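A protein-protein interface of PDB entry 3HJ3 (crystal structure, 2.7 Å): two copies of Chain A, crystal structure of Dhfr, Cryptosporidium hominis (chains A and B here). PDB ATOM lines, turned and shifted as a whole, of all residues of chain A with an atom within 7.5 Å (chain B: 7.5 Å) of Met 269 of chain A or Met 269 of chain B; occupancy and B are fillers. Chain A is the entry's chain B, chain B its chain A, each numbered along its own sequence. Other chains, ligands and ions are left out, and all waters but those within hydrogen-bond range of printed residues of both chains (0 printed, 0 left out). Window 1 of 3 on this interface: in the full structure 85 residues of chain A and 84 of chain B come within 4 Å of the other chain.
The guanidinium group (NH2) of Arg 271 of chain A is in hydrogen-bond range of the side-chain amide oxygen (OE1) of Gln 268 of chain B, 3.1 Å away. The guanidinium group (NH2) of Arg 271 of chain B lies within hydrogen-bond range of the side-chain amide oxygen (OE1) of Gln 268 of chain A (3.4 Å). The backbone carbonyl oxygen of Gly 267 of chain A lies close to the guanidinium group of Arg 271 of chain B (2.4 Å). NH2 of Arg 271 of chain A lies close to O of Gly 267 of chain B (2.3 Å).
Gly 267 of chain A touches Arg 271 of chain B, and with the chains exchanged Arg 271 of chain A touches Gly 267 of chain B. Gly 267 of chain A touches Phe 459 of chain B, but with the chains exchanged Phe 459 of chain A does not touch Gly 267 of chain B (4.1 Å). Gln 268 of chain A touches Arg 271 of chain B, and with the chains exchanged Arg 271 of chain A touches Gln 268 of chain B. Gln 268 of chain A touches Phe 459 of chain B, but with the chains exchanged Phe 459 of chain A does not touch Gln 268 of chain B (4.03 Å). Positions printed for both chains: 239, 240, 243, 246, 267, 268, 269, 270, 271, 272, 457, 458, 459, 460 and 463.
Of the 15 printed residues of chain A, 5 touch a printed residue of chain B. Printed residues of chain A that touch a printed residue of chain B: Gly 267, Gln 268, Met 269, Arg 271 and Phe 459. Hydrophobic or aromatic side chains of chain A within 4 Å of the printed part of chain B: Met 269 and Phe 459. Of the 16 printed residues of chain B, 5 touch a printed residue of chain A. Printed residues of chain B that touch a printed residue of chain A: Gly 267, Gln 268, Met 269, Arg 271 and Phe 459. Hydrophobic or aromatic side chains of chain B within 4 Å of the printed part of chain A: Met 269 and Phe 459. Among the printed residues, 8 pairs touch across the chains. Among the printed residues, no Asp or Glu carboxylate lies within 4 Å of a Lys or Arg side-chain nitrogen of the other chain.
The side-chain amide oxygen (OE1) of Gln 239 of chain B sits at hydrogen-bond distance from the backbone NH (N) of Arg 271 of chain B, 2.9 Å away. The guanidinium group (NH1) of Arg 246 of chain B lies close to the side-chain amide nitrogen (NE2) of Gln 268 of chain B (2.7 Å). The backbone NH (N) of Gly 267 of chain B sits at hydrogen-bond distance from the backbone carbonyl oxygen (O) of Gly 461 of chain B (3.0 Å). N of Arg 271 of chain A is in hydrogen-bond range of OE1 of Gln 239 of chain A (3.0 Å). O of Ile 460 of chain A lies close to N of Gly 267 of chain A (3.3 Å). O of Gln 268 of chain A is in hydrogen-bond range of N of Ile 460 of chain A, 2.8 Å away.
Printed residues of chain B within 4 Å of Gln 268 of chain A: Arg 271 (3.4 Å) and Phe 459 (3.8 Å). Of chain B, only Met 269 (3.7 Å) comes within 4 Å of Met 269 of chain A. Printed residues of chain A within 4 Å of Gly 267 of chain B: Arg 271 (2.3 Å). Met 269 of chain B touches one residue of chain A. Printed residues of chain A within 4 Å of Arg 271 of chain B: Gly 267 (2.4 Å) and Gln 268 (3.4 Å). Of the printed residues of chain A, Phe 459 of chain B touches Gly 267, Gln 268 and Phe 459.
CA of Gly 267 of chain A touches CZ of Phe 459 of chain B, at 3.99 Å. Gln 268 of chain A touches Phe 459 of chain B. Met 269 of chain B touches Met 269 of chain A (CG to CE, 3.7 Å). Phe 459 of chain A touches Phe 459 of chain B (CD2 to CD2, 3.1 Å).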
ATOM      1  N   GLN A 239     -10.611  33.320 -17.912  1.00  0.00           N
ATOM      2  CA  GLN A 239      -9.774  32.311 -18.470  1.00  0.00           C
ATOM      3  C   GLN A 239      -9.631  32.500 -19.988  1.00  0.00           C
ATOM      4  O   GLN A 239      -8.543  32.385 -20.531  1.00  0.00           O
ATOM      5  CB  GLN A 239     -10.325  30.958 -18.146  1.00  0.00           C
ATOM      6  CG  GLN A 239     -10.449  30.733 -16.667  1.00  0.00           C
ATOM      7  CD  GLN A 239      -9.235  30.059 -16.020  1.00  0.00           C
ATOM      8  OE1 GLN A 239      -8.629  29.102 -16.551  1.00  0.00           O
ATOM      9  NE2 GLN A 239      -8.904  30.522 -14.837  1.00  0.00           N
ATOM     10  N   TYR A 240     -10.717  32.822 -20.675  1.00  0.00           N
ATOM     11  CA  TYR A 240     -10.646  33.150 -22.099  1.00  0.00           C
ATOM     12  C   TYR A 240      -9.927  34.482 -22.335  1.00  0.00           C
ATOM     13  O   TYR A 240      -9.071  34.581 -23.192  1.00  0.00           O
ATOM     14  CB  TYR A 240     -12.055  33.174 -22.733  1.00  0.00           C
ATOM     15  CG  TYR A 240     -12.072  33.728 -24.123  1.00  0.00           C
ATOM     16  CD1 TYR A 240     -12.498  35.012 -24.364  1.00  0.00           C
ATOM     17  CD2 TYR A 240     -11.620  32.944 -25.214  1.00  0.00           C
ATOM     18  CE1 TYR A 240     -12.486  35.536 -25.711  1.00  0.00           C
ATOM     19  CE2 TYR A 240     -11.597  33.406 -26.557  1.00  0.00           C
ATOM     20  CZ  TYR A 240     -12.034  34.697 -26.807  1.00  0.00           C
ATOM     21  OH  TYR A 240     -12.023  35.144 -28.123  1.00  0.00           O
ATOM     22  N   LEU A 243      -6.125  34.495 -21.690  1.00  0.00           N
ATOM     23  CA  LEU A 243      -5.398  33.762 -22.695  1.00  0.00           C
ATOM     24  C   LEU A 243      -5.143  34.702 -23.885  1.00  0.00           C
ATOM     25  O   LEU A 243      -4.035  34.735 -24.462  1.00  0.00           O
ATOM     26  CB  LEU A 243      -6.159  32.523 -23.166  1.00  0.00           C
ATOM     27  CG  LEU A 243      -5.551  31.731 -24.344  1.00  0.00           C
ATOM     28  CD1 LEU A 243      -4.081  31.390 -24.197  1.00  0.00           C
ATOM     29  CD2 LEU A 243      -6.296  30.455 -24.437  1.00  0.00           C
ATOM     30  N   ARG A 246      -2.531  37.115 -23.563  1.00  0.00           N
ATOM     31  CA  ARG A 246      -1.259  36.442 -23.326  1.00  0.00           C
ATOM     32  C   ARG A 246      -0.520  36.186 -24.635  1.00  0.00           C
ATOM     33  O   ARG A 246       0.697  36.353 -24.715  1.00  0.00           O
ATOM     34  CB  ARG A 246      -1.481  35.124 -22.581  1.00  0.00           C
ATOM     35  CG  ARG A 246      -1.509  35.263 -21.069  1.00  0.00           C
ATOM     36  CD  ARG A 246      -1.087  33.972 -20.387  1.00  0.00           C
ATOM     37  NE  ARG A 246      -2.009  32.877 -20.672  1.00  0.00           N
ATOM     38  CZ  ARG A 246      -3.150  32.672 -20.022  1.00  0.00           C
ATOM     39  NH1 ARG A 246      -3.928  31.650 -20.348  1.00  0.00           N
ATOM     40  NH2 ARG A 246      -3.514  33.491 -19.043  1.00  0.00           N
ATOM     41  N   GLY A 267       0.717  25.664 -25.858  1.00  0.00           N
ATOM     42  CA  GLY A 267       0.451  25.061 -24.534  1.00  0.00           C
ATOM     43  C   GLY A 267      -0.179  25.988 -23.507  1.00  0.00           C
ATOM     44  O   GLY A 267       0.479  26.771 -22.903  1.00  0.00           O
ATOM     45  N   GLN A 268      -1.478  25.916 -23.334  1.00  0.00           N
ATOM     46  CA  GLN A 268      -2.207  26.893 -22.530  1.00  0.00           C
ATOM     47  C   GLN A 268      -3.508  26.236 -22.203  1.00  0.00           C
ATOM     48  O   GLN A 268      -3.921  25.281 -22.855  1.00  0.00           O
ATOM     49  CB  GLN A 268      -2.547  28.154 -23.356  1.00  0.00           C
ATOM     50  CG  GLN A 268      -1.417  29.082 -23.686  1.00  0.00           C
ATOM     51  CD  GLN A 268      -0.945  29.880 -22.467  1.00  0.00           C
ATOM     52  OE1 GLN A 268       0.266  30.007 -22.213  1.00  0.00           O
ATOM     53  NE2 GLN A 268      -1.882  30.394 -21.699  1.00  0.00           N
ATOM     54  N   MET A 269      -4.200  26.778 -21.220  1.00  0.00           N
ATOM     55  CA  MET A 269      -5.391  26.119 -20.770  1.00  0.00           C
ATOM     56  C   MET A 269      -6.408  27.057 -20.234  1.00  0.00           C
ATOM     57  O   MET A 269      -6.060  28.154 -19.856  1.00  0.00           O
ATOM     58  CB  MET A 269      -5.042  25.041 -19.735  1.00  0.00           C
ATOM     59  CG  MET A 269      -4.791  25.515 -18.337  1.00  0.00           C
ATOM     60  SD  MET A 269      -5.194  24.138 -17.204  1.00  0.00           S
ATOM     61  CE  MET A 269      -4.453  24.791 -15.698  1.00  0.00           C
ATOM     62  N   MET A 270      -7.669  26.604 -20.202  1.00  0.00           N
ATOM     63  CA  MET A 270      -8.785  27.338 -19.602  1.00  0.00           C
ATOM     64  C   MET A 270      -9.692  26.387 -18.807  1.00  0.00           C
ATOM     65  O   MET A 270      -9.953  25.294 -19.267  1.00  0.00           O
ATOM     66  CB  MET A 270      -9.611  28.033 -20.682  1.00  0.00           C
ATOM     67  CG  MET A 270      -8.843  28.829 -21.714  1.00  0.00           C
ATOM     68  SD  MET A 270      -9.944  29.612 -22.900  1.00  0.00           S
ATOM     69  CE  MET A 270     -10.201  28.356 -24.106  1.00  0.00           C
ATOM     70  N   ARG A 271     -10.166  26.815 -17.642  1.00  0.00           N
ATOM     71  CA  ARG A 271     -11.185  26.093 -16.892  1.00  0.00           C
ATOM     72  C   ARG A 271     -12.495  26.911 -16.915  1.00  0.00           C
ATOM     73  O   ARG A 271     -12.454  28.114 -17.054  1.00  0.00           O
ATOM     74  CB  ARG A 271     -10.797  25.926 -15.442  1.00  0.00           C
ATOM     75  CG  ARG A 271      -9.804  24.962 -15.147  1.00  0.00           C
ATOM     76  CD  ARG A 271     -10.296  24.021 -14.006  1.00  0.00           C
ATOM     77  NE  ARG A 271      -9.397  22.837 -13.814  1.00  0.00           N
ATOM     78  CZ  ARG A 271      -8.103  22.995 -13.580  1.00  0.00           C
ATOM     79  NH1 ARG A 271      -7.594  24.224 -13.527  1.00  0.00           N
ATOM     80  NH2 ARG A 271      -7.311  21.975 -13.411  1.00  0.00           N
ATOM     81  N   PHE A 272     -13.636  26.245 -16.790  1.00  0.00           N
ATOM     82  CA  PHE A 272     -14.933  26.902 -16.739  1.00  0.00           C
ATOM     83  C   PHE A 272     -15.821  26.060 -15.851  1.00  0.00           C
ATOM     84  O   PHE A 272     -15.897  24.859 -16.029  1.00  0.00           O
ATOM     85  CB  PHE A 272     -15.567  26.977 -18.146  1.00  0.00           C
ATOM     86  CG  PHE A 272     -14.822  27.864 -19.119  1.00  0.00           C
ATOM     87  CD1 PHE A 272     -15.038  29.224 -19.125  1.00  0.00           C
ATOM     88  CD2 PHE A 272     -13.895  27.323 -20.000  1.00  0.00           C
ATOM     89  CE1 PHE A 272     -14.379  30.027 -19.986  1.00  0.00           C
ATOM     90  CE2 PHE A 272     -13.179  28.136 -20.914  1.00  0.00           C
ATOM     91  CZ  PHE A 272     -13.412  29.481 -20.905  1.00  0.00           C
ATOM     92  N   ALA A 457     -12.493  21.763 -18.780  1.00  0.00           N
ATOM     93  CA  ALA A 457     -11.127  22.233 -18.974  1.00  0.00           C
ATOM     94  C   ALA A 457     -10.698  22.094 -20.431  1.00  0.00           C
ATOM     95  O   ALA A 457     -11.013  21.102 -21.089  1.00  0.00           O
ATOM     96  CB  ALA A 457     -10.172  21.479 -18.063  1.00  0.00           C
ATOM     97  N   ILE A 458      -9.978  23.094 -20.929  1.00  0.00           N
ATOM     98  CA  ILE A 458      -9.627  23.155 -22.343  1.00  0.00           C
ATOM     99  C   ILE A 458      -8.126  23.358 -22.529  1.00  0.00           C
ATOM    100  O   ILE A 458      -7.576  24.388 -22.141  1.00  0.00           O
ATOM    101  CB  ILE A 458     -10.382  24.287 -23.064  1.00  0.00           C
ATOM    102  CG1 ILE A 458     -11.870  23.948 -23.174  1.00  0.00           C
ATOM    103  CG2 ILE A 458      -9.784  24.533 -24.441  1.00  0.00           C
ATOM    104  CD1 ILE A 458     -12.643  24.882 -24.079  1.00  0.00           C
ATOM    105  N   PHE A 459      -7.471  22.369 -23.129  1.00  0.00           N
ATOM    106  CA  PHE A 459      -6.064  22.435 -23.364  1.00  0.00           C
ATOM    107  C   PHE A 459      -5.736  22.787 -24.814  1.00  0.00           C
ATOM    108  O   PHE A 459      -6.193  22.135 -25.708  1.00  0.00           O
ATOM    109  CB  PHE A 459      -5.499  21.131 -22.941  1.00  0.00           C
ATOM    110  CG  PHE A 459      -5.866  20.765 -21.525  1.00  0.00           C
ATOM    111  CD1 PHE A 459      -6.607  19.649 -21.264  1.00  0.00           C
ATOM    112  CD2 PHE A 459      -5.440  21.535 -20.457  1.00  0.00           C
ATOM    113  CE1 PHE A 459      -6.912  19.279 -19.972  1.00  0.00           C
ATOM    114  CE2 PHE A 459      -5.745  21.188 -19.148  1.00  0.00           C
ATOM    115  CZ  PHE A 459      -6.498  20.048 -18.908  1.00  0.00           C
ATOM    116  N   ILE A 460      -5.008  23.876 -25.036  1.00  0.00           N
ATOM    117  CA  ILE A 460      -4.704  24.355 -26.383  1.00  0.00           C
ATOM    118  C   ILE A 460      -3.246  24.067 -26.706  1.00  0.00           C
ATOM    119  O   ILE A 460      -2.320  24.383 -25.911  1.00  0.00           O
ATOM    120  CB  ILE A 460      -4.868  25.915 -26.524  1.00  0.00           C
ATOM    121  CG1 ILE A 460      -6.042  26.446 -25.722  1.00  0.00           C
ATOM    122  CG2 ILE A 460      -5.040  26.285 -27.949  1.00  0.00           C
ATOM    123  CD1 ILE A 460      -7.217  25.688 -25.996  1.00  0.00           C
ATOM    124  N   ALA A 463      -2.293  28.022 -29.653  1.00  0.00           N
ATOM    125  CA  ALA A 463      -3.196  29.133 -29.382  1.00  0.00           C
ATOM    126  C   ALA A 463      -2.766  30.391 -30.131  1.00  0.00           C
ATOM    127  O   ALA A 463      -1.704  30.952 -29.861  1.00  0.00           O
ATOM    128  CB  ALA A 463      -3.271  29.404 -27.886  1.00  0.00           C
ATOM    129  N   GLN B 239       6.196  21.945 -10.294  1.00  0.00           N
ATOM    130  CA  GLN B 239       5.036  21.683 -11.074  1.00  0.00           C
ATOM    131  C   GLN B 239       4.588  20.273 -10.828  1.00  0.00           C
ATOM    132  O   GLN B 239       3.389  20.003 -10.919  1.00  0.00           O
ATOM    133  CB  GLN B 239       5.308  21.899 -12.547  1.00  0.00           C
ATOM    134  CG  GLN B 239       5.673  23.272 -12.753  1.00  0.00           C
ATOM    135  CD  GLN B 239       4.556  24.121 -13.254  1.00  0.00           C
ATOM    136  OE1 GLN B 239       3.818  23.744 -14.167  1.00  0.00           O
ATOM    137  NE2 GLN B 239       4.455  25.316 -12.715  1.00  0.00           N
ATOM    138  N   TYR B 240       5.525  19.379 -10.514  1.00  0.00           N
ATOM    139  CA  TYR B 240       5.196  17.966 -10.287  1.00  0.00           C
ATOM    140  C   TYR B 240       4.793  17.753  -8.840  1.00  0.00           C
ATOM    141  O   TYR B 240       3.865  17.001  -8.550  1.00  0.00           O
ATOM    142  CB  TYR B 240       6.340  17.010 -10.666  1.00  0.00           C
ATOM    143  CG  TYR B 240       6.120  15.621 -10.073  1.00  0.00           C
ATOM    144  CD1 TYR B 240       6.746  15.256  -8.881  1.00  0.00           C
ATOM    145  CD2 TYR B 240       5.280  14.690 -10.680  1.00  0.00           C
ATOM    146  CE1 TYR B 240       6.539  14.011  -8.300  1.00  0.00           C
ATOM    147  CE2 TYR B 240       5.070  13.414 -10.131  1.00  0.00           C
ATOM    148  CZ  TYR B 240       5.681  13.078  -8.937  1.00  0.00           C
ATOM    149  OH  TYR B 240       5.484  11.797  -8.361  1.00  0.00           O
ATOM    150  N   LEU B 243       1.331  19.298  -7.986  1.00  0.00           N
ATOM    151  CA  LEU B 243       0.294  18.461  -8.516  1.00  0.00           C
ATOM    152  C   LEU B 243      -0.019  17.380  -7.485  1.00  0.00           C
ATOM    153  O   LEU B 243      -1.168  17.150  -7.087  1.00  0.00           O
ATOM    154  CB  LEU B 243       0.675  17.868  -9.886  1.00  0.00           C
ATOM    155  CG  LEU B 243      -0.418  16.950 -10.438  1.00  0.00           C
ATOM    156  CD1 LEU B 243      -1.825  17.601 -10.479  1.00  0.00           C
ATOM    157  CD2 LEU B 243      -0.022  16.449 -11.762  1.00  0.00           C
ATOM    158  N   ARG B 246      -2.009  18.924  -4.627  1.00  0.00           N
ATOM    159  CA  ARG B 246      -3.368  19.204  -5.019  1.00  0.00           C
ATOM    160  C   ARG B 246      -4.215  17.929  -4.958  1.00  0.00           C
ATOM    161  O   ARG B 246      -5.408  18.005  -4.558  1.00  0.00           O
ATOM    162  CB  ARG B 246      -3.463  19.874  -6.404  1.00  0.00           C
ATOM    163  CG  ARG B 246      -3.065  21.386  -6.320  1.00  0.00           C
ATOM    164  CD  ARG B 246      -3.358  22.227  -7.527  1.00  0.00           C
ATOM    165  NE  ARG B 246      -2.862  21.595  -8.762  1.00  0.00           N
ATOM    166  CZ  ARG B 246      -1.639  21.773  -9.271  1.00  0.00           C
ATOM    167  NH1 ARG B 246      -1.275  21.113 -10.371  1.00  0.00           N
ATOM    168  NH2 ARG B 246      -0.784  22.597  -8.676  1.00  0.00           N
ATOM    169  N   GLY B 267      -8.276  16.970 -14.772  1.00  0.00           N
ATOM    170  CA  GLY B 267      -7.931  18.203 -15.478  1.00  0.00           C
ATOM    171  C   GLY B 267      -6.823  18.927 -14.723  1.00  0.00           C
ATOM    172  O   GLY B 267      -7.076  19.761 -13.884  1.00  0.00           O
ATOM    173  N   GLN B 268      -5.578  18.583 -14.986  1.00  0.00           N
ATOM    174  CA  GLN B 268      -4.494  19.273 -14.380  1.00  0.00           C
ATOM    175  C   GLN B 268      -3.434  19.481 -15.445  1.00  0.00           C
ATOM    176  O   GLN B 268      -3.481  18.871 -16.514  1.00  0.00           O
ATOM    177  CB  GLN B 268      -3.959  18.422 -13.245  1.00  0.00           C
ATOM    178  CG  GLN B 268      -4.812  18.458 -11.990  1.00  0.00           C
ATOM    179  CD  GLN B 268      -4.900  19.858 -11.357  1.00  0.00           C
ATOM    180  OE1 GLN B 268      -5.993  20.383 -11.142  1.00  0.00           O
ATOM    181  NE2 GLN B 268      -3.769  20.454 -11.075  1.00  0.00           N
ATOM    182  N   MET B 269      -2.440  20.292 -15.133  1.00  0.00           N
ATOM    183  CA  MET B 269      -1.357  20.480 -16.050  1.00  0.00           C
ATOM    184  C   MET B 269      -0.020  20.731 -15.361  1.00  0.00           C
ATOM    185  O   MET B 269       0.017  21.117 -14.211  1.00  0.00           O
ATOM    186  CB  MET B 269      -1.703  21.619 -16.982  1.00  0.00           C
ATOM    187  CG  MET B 269      -1.301  22.993 -16.543  1.00  0.00           C
ATOM    188  SD  MET B 269      -1.051  23.922 -18.052  1.00  0.00           S
ATOM    189  CE  MET B 269      -0.761  25.594 -17.404  1.00  0.00           C
ATOM    190  N   MET B 270       1.068  20.473 -16.084  1.00  0.00           N
ATOM    191  CA  MET B 270       2.448  20.669 -15.632  1.00  0.00           C
ATOM    192  C   MET B 270       3.297  21.191 -16.806  1.00  0.00           C
ATOM    193  O   MET B 270       3.075  20.852 -17.995  1.00  0.00           O
ATOM    194  CB  MET B 270       3.068  19.368 -15.187  1.00  0.00           C
ATOM    195  CG  MET B 270       2.548  18.726 -14.003  1.00  0.00           C
ATOM    196  SD  MET B 270       3.495  17.231 -13.523  1.00  0.00           S
ATOM    197  CE  MET B 270       2.962  16.042 -14.827  1.00  0.00           C
ATOM    198  N   ARG B 271       4.293  21.986 -16.463  1.00  0.00           N
ATOM    199  CA  ARG B 271       5.171  22.631 -17.438  1.00  0.00           C
ATOM    200  C   ARG B 271       6.598  22.471 -17.042  1.00  0.00           C
ATOM    201  O   ARG B 271       6.960  22.627 -15.871  1.00  0.00           O
ATOM    202  CB  ARG B 271       4.944  24.132 -17.490  1.00  0.00           C
ATOM    203  CG  ARG B 271       3.944  24.564 -18.442  1.00  0.00           C
ATOM    204  CD  ARG B 271       4.315  25.935 -18.956  1.00  0.00           C
ATOM    205  NE  ARG B 271       3.401  26.295 -20.027  1.00  0.00           N
ATOM    206  CZ  ARG B 271       2.266  26.914 -19.797  1.00  0.00           C
ATOM    207  NH1 ARG B 271       1.936  27.267 -18.561  1.00  0.00           N
ATOM    208  NH2 ARG B 271       1.468  27.167 -20.796  1.00  0.00           N
ATOM    209  N   PHE B 272       7.427  22.233 -18.034  1.00  0.00           N
ATOM    210  CA  PHE B 272       8.840  22.077 -17.776  1.00  0.00           C
ATOM    211  C   PHE B 272       9.684  22.747 -18.832  1.00  0.00           C
ATOM    212  O   PHE B 272       9.399  22.649 -20.044  1.00  0.00           O
ATOM    213  CB  PHE B 272       9.138  20.606 -17.734  1.00  0.00           C
ATOM    214  CG  PHE B 272       8.366  19.851 -16.684  1.00  0.00           C
ATOM    215  CD1 PHE B 272       8.831  19.828 -15.361  1.00  0.00           C
ATOM    216  CD2 PHE B 272       7.236  19.098 -17.024  1.00  0.00           C
ATOM    217  CE1 PHE B 272       8.201  19.080 -14.396  1.00  0.00           C
ATOM    218  CE2 PHE B 272       6.555  18.302 -16.029  1.00  0.00           C
ATOM    219  CZ  PHE B 272       7.055  18.309 -14.717  1.00  0.00           C
ATOM    220  N   ALA B 457       4.832  20.563 -21.955  1.00  0.00           N
ATOM    221  CA  ALA B 457       3.648  20.832 -21.150  1.00  0.00           C
ATOM    222  C   ALA B 457       2.905  19.538 -21.062  1.00  0.00           C
ATOM    223  O   ALA B 457       2.697  18.899 -22.081  1.00  0.00           O
ATOM    224  CB  ALA B 457       2.755  21.910 -21.829  1.00  0.00           C
ATOM    225  N   ILE B 458       2.529  19.116 -19.865  1.00  0.00           N
ATOM    226  CA  ILE B 458       1.748  17.876 -19.800  1.00  0.00           C
ATOM    227  C   ILE B 458       0.335  18.177 -19.285  1.00  0.00           C
ATOM    228  O   ILE B 458       0.198  18.827 -18.243  1.00  0.00           O
ATOM    229  CB  ILE B 458       2.453  16.819 -18.970  1.00  0.00           C
ATOM    230  CG1 ILE B 458       3.791  16.520 -19.612  1.00  0.00           C
ATOM    231  CG2 ILE B 458       1.637  15.538 -18.903  1.00  0.00           C
ATOM    232  CD1 ILE B 458       4.748  15.787 -18.703  1.00  0.00           C
ATOM    233  N   PHE B 459      -0.689  17.772 -20.050  1.00  0.00           N
ATOM    234  CA  PHE B 459      -2.080  17.988 -19.657  1.00  0.00           C
ATOM    235  C   PHE B 459      -2.655  16.694 -19.167  1.00  0.00           C
ATOM    236  O   PHE B 459      -2.560  15.704 -19.876  1.00  0.00           O
ATOM    237  CB  PHE B 459      -2.882  18.544 -20.804  1.00  0.00           C
ATOM    238  CG  PHE B 459      -2.368  19.850 -21.309  1.00  0.00           C
ATOM    239  CD1 PHE B 459      -1.875  19.961 -22.599  1.00  0.00           C
ATOM    240  CD2 PHE B 459      -2.346  20.962 -20.489  1.00  0.00           C
ATOM    241  CE1 PHE B 459      -1.349  21.152 -23.083  1.00  0.00           C
ATOM    242  CE2 PHE B 459      -1.824  22.203 -20.971  1.00  0.00           C
ATOM    243  CZ  PHE B 459      -1.315  22.273 -22.287  1.00  0.00           C
ATOM    244  N   ILE B 460      -3.185  16.663 -17.946  1.00  0.00           N
ATOM    245  CA  ILE B 460      -3.626  15.381 -17.394  1.00  0.00           C
ATOM    246  C   ILE B 460      -5.119  15.249 -17.291  1.00  0.00           C
ATOM    247  O   ILE B 460      -5.828  16.198 -16.921  1.00  0.00           O
ATOM    248  CB  ILE B 460      -3.131  15.166 -15.992  1.00  0.00           C
ATOM    249  CG1 ILE B 460      -1.689  15.698 -15.870  1.00  0.00           C
ATOM    250  CG2 ILE B 460      -3.361  13.697 -15.606  1.00  0.00           C
ATOM    251  CD1 ILE B 460      -0.672  14.637 -15.937  1.00  0.00           C
ATOM    252  N   GLY B 461      -5.601  14.039 -17.525  1.00  0.00           N
ATOM    253  CA  GLY B 461      -7.022  13.757 -17.330  1.00  0.00           C
ATOM    254  C   GLY B 461      -7.248  13.320 -15.897  1.00  0.00           C
ATOM    255  O   GLY B 461      -7.343  14.125 -14.986  1.00  0.00           O
ATOM    256  N   ALA B 463      -5.882  12.506 -12.896  1.00  0.00           N
ATOM    257  CA  ALA B 463      -4.617  12.592 -12.159  1.00  0.00           C
ATOM    258  C   ALA B 463      -4.824  11.981 -10.815  1.00  0.00           C
ATOM    259  O   ALA B 463      -5.558  12.520 -10.036  1.00  0.00           O
ATOM    260  CB  ALA B 463      -4.173  14.072 -12.022  1.00  0.00           C
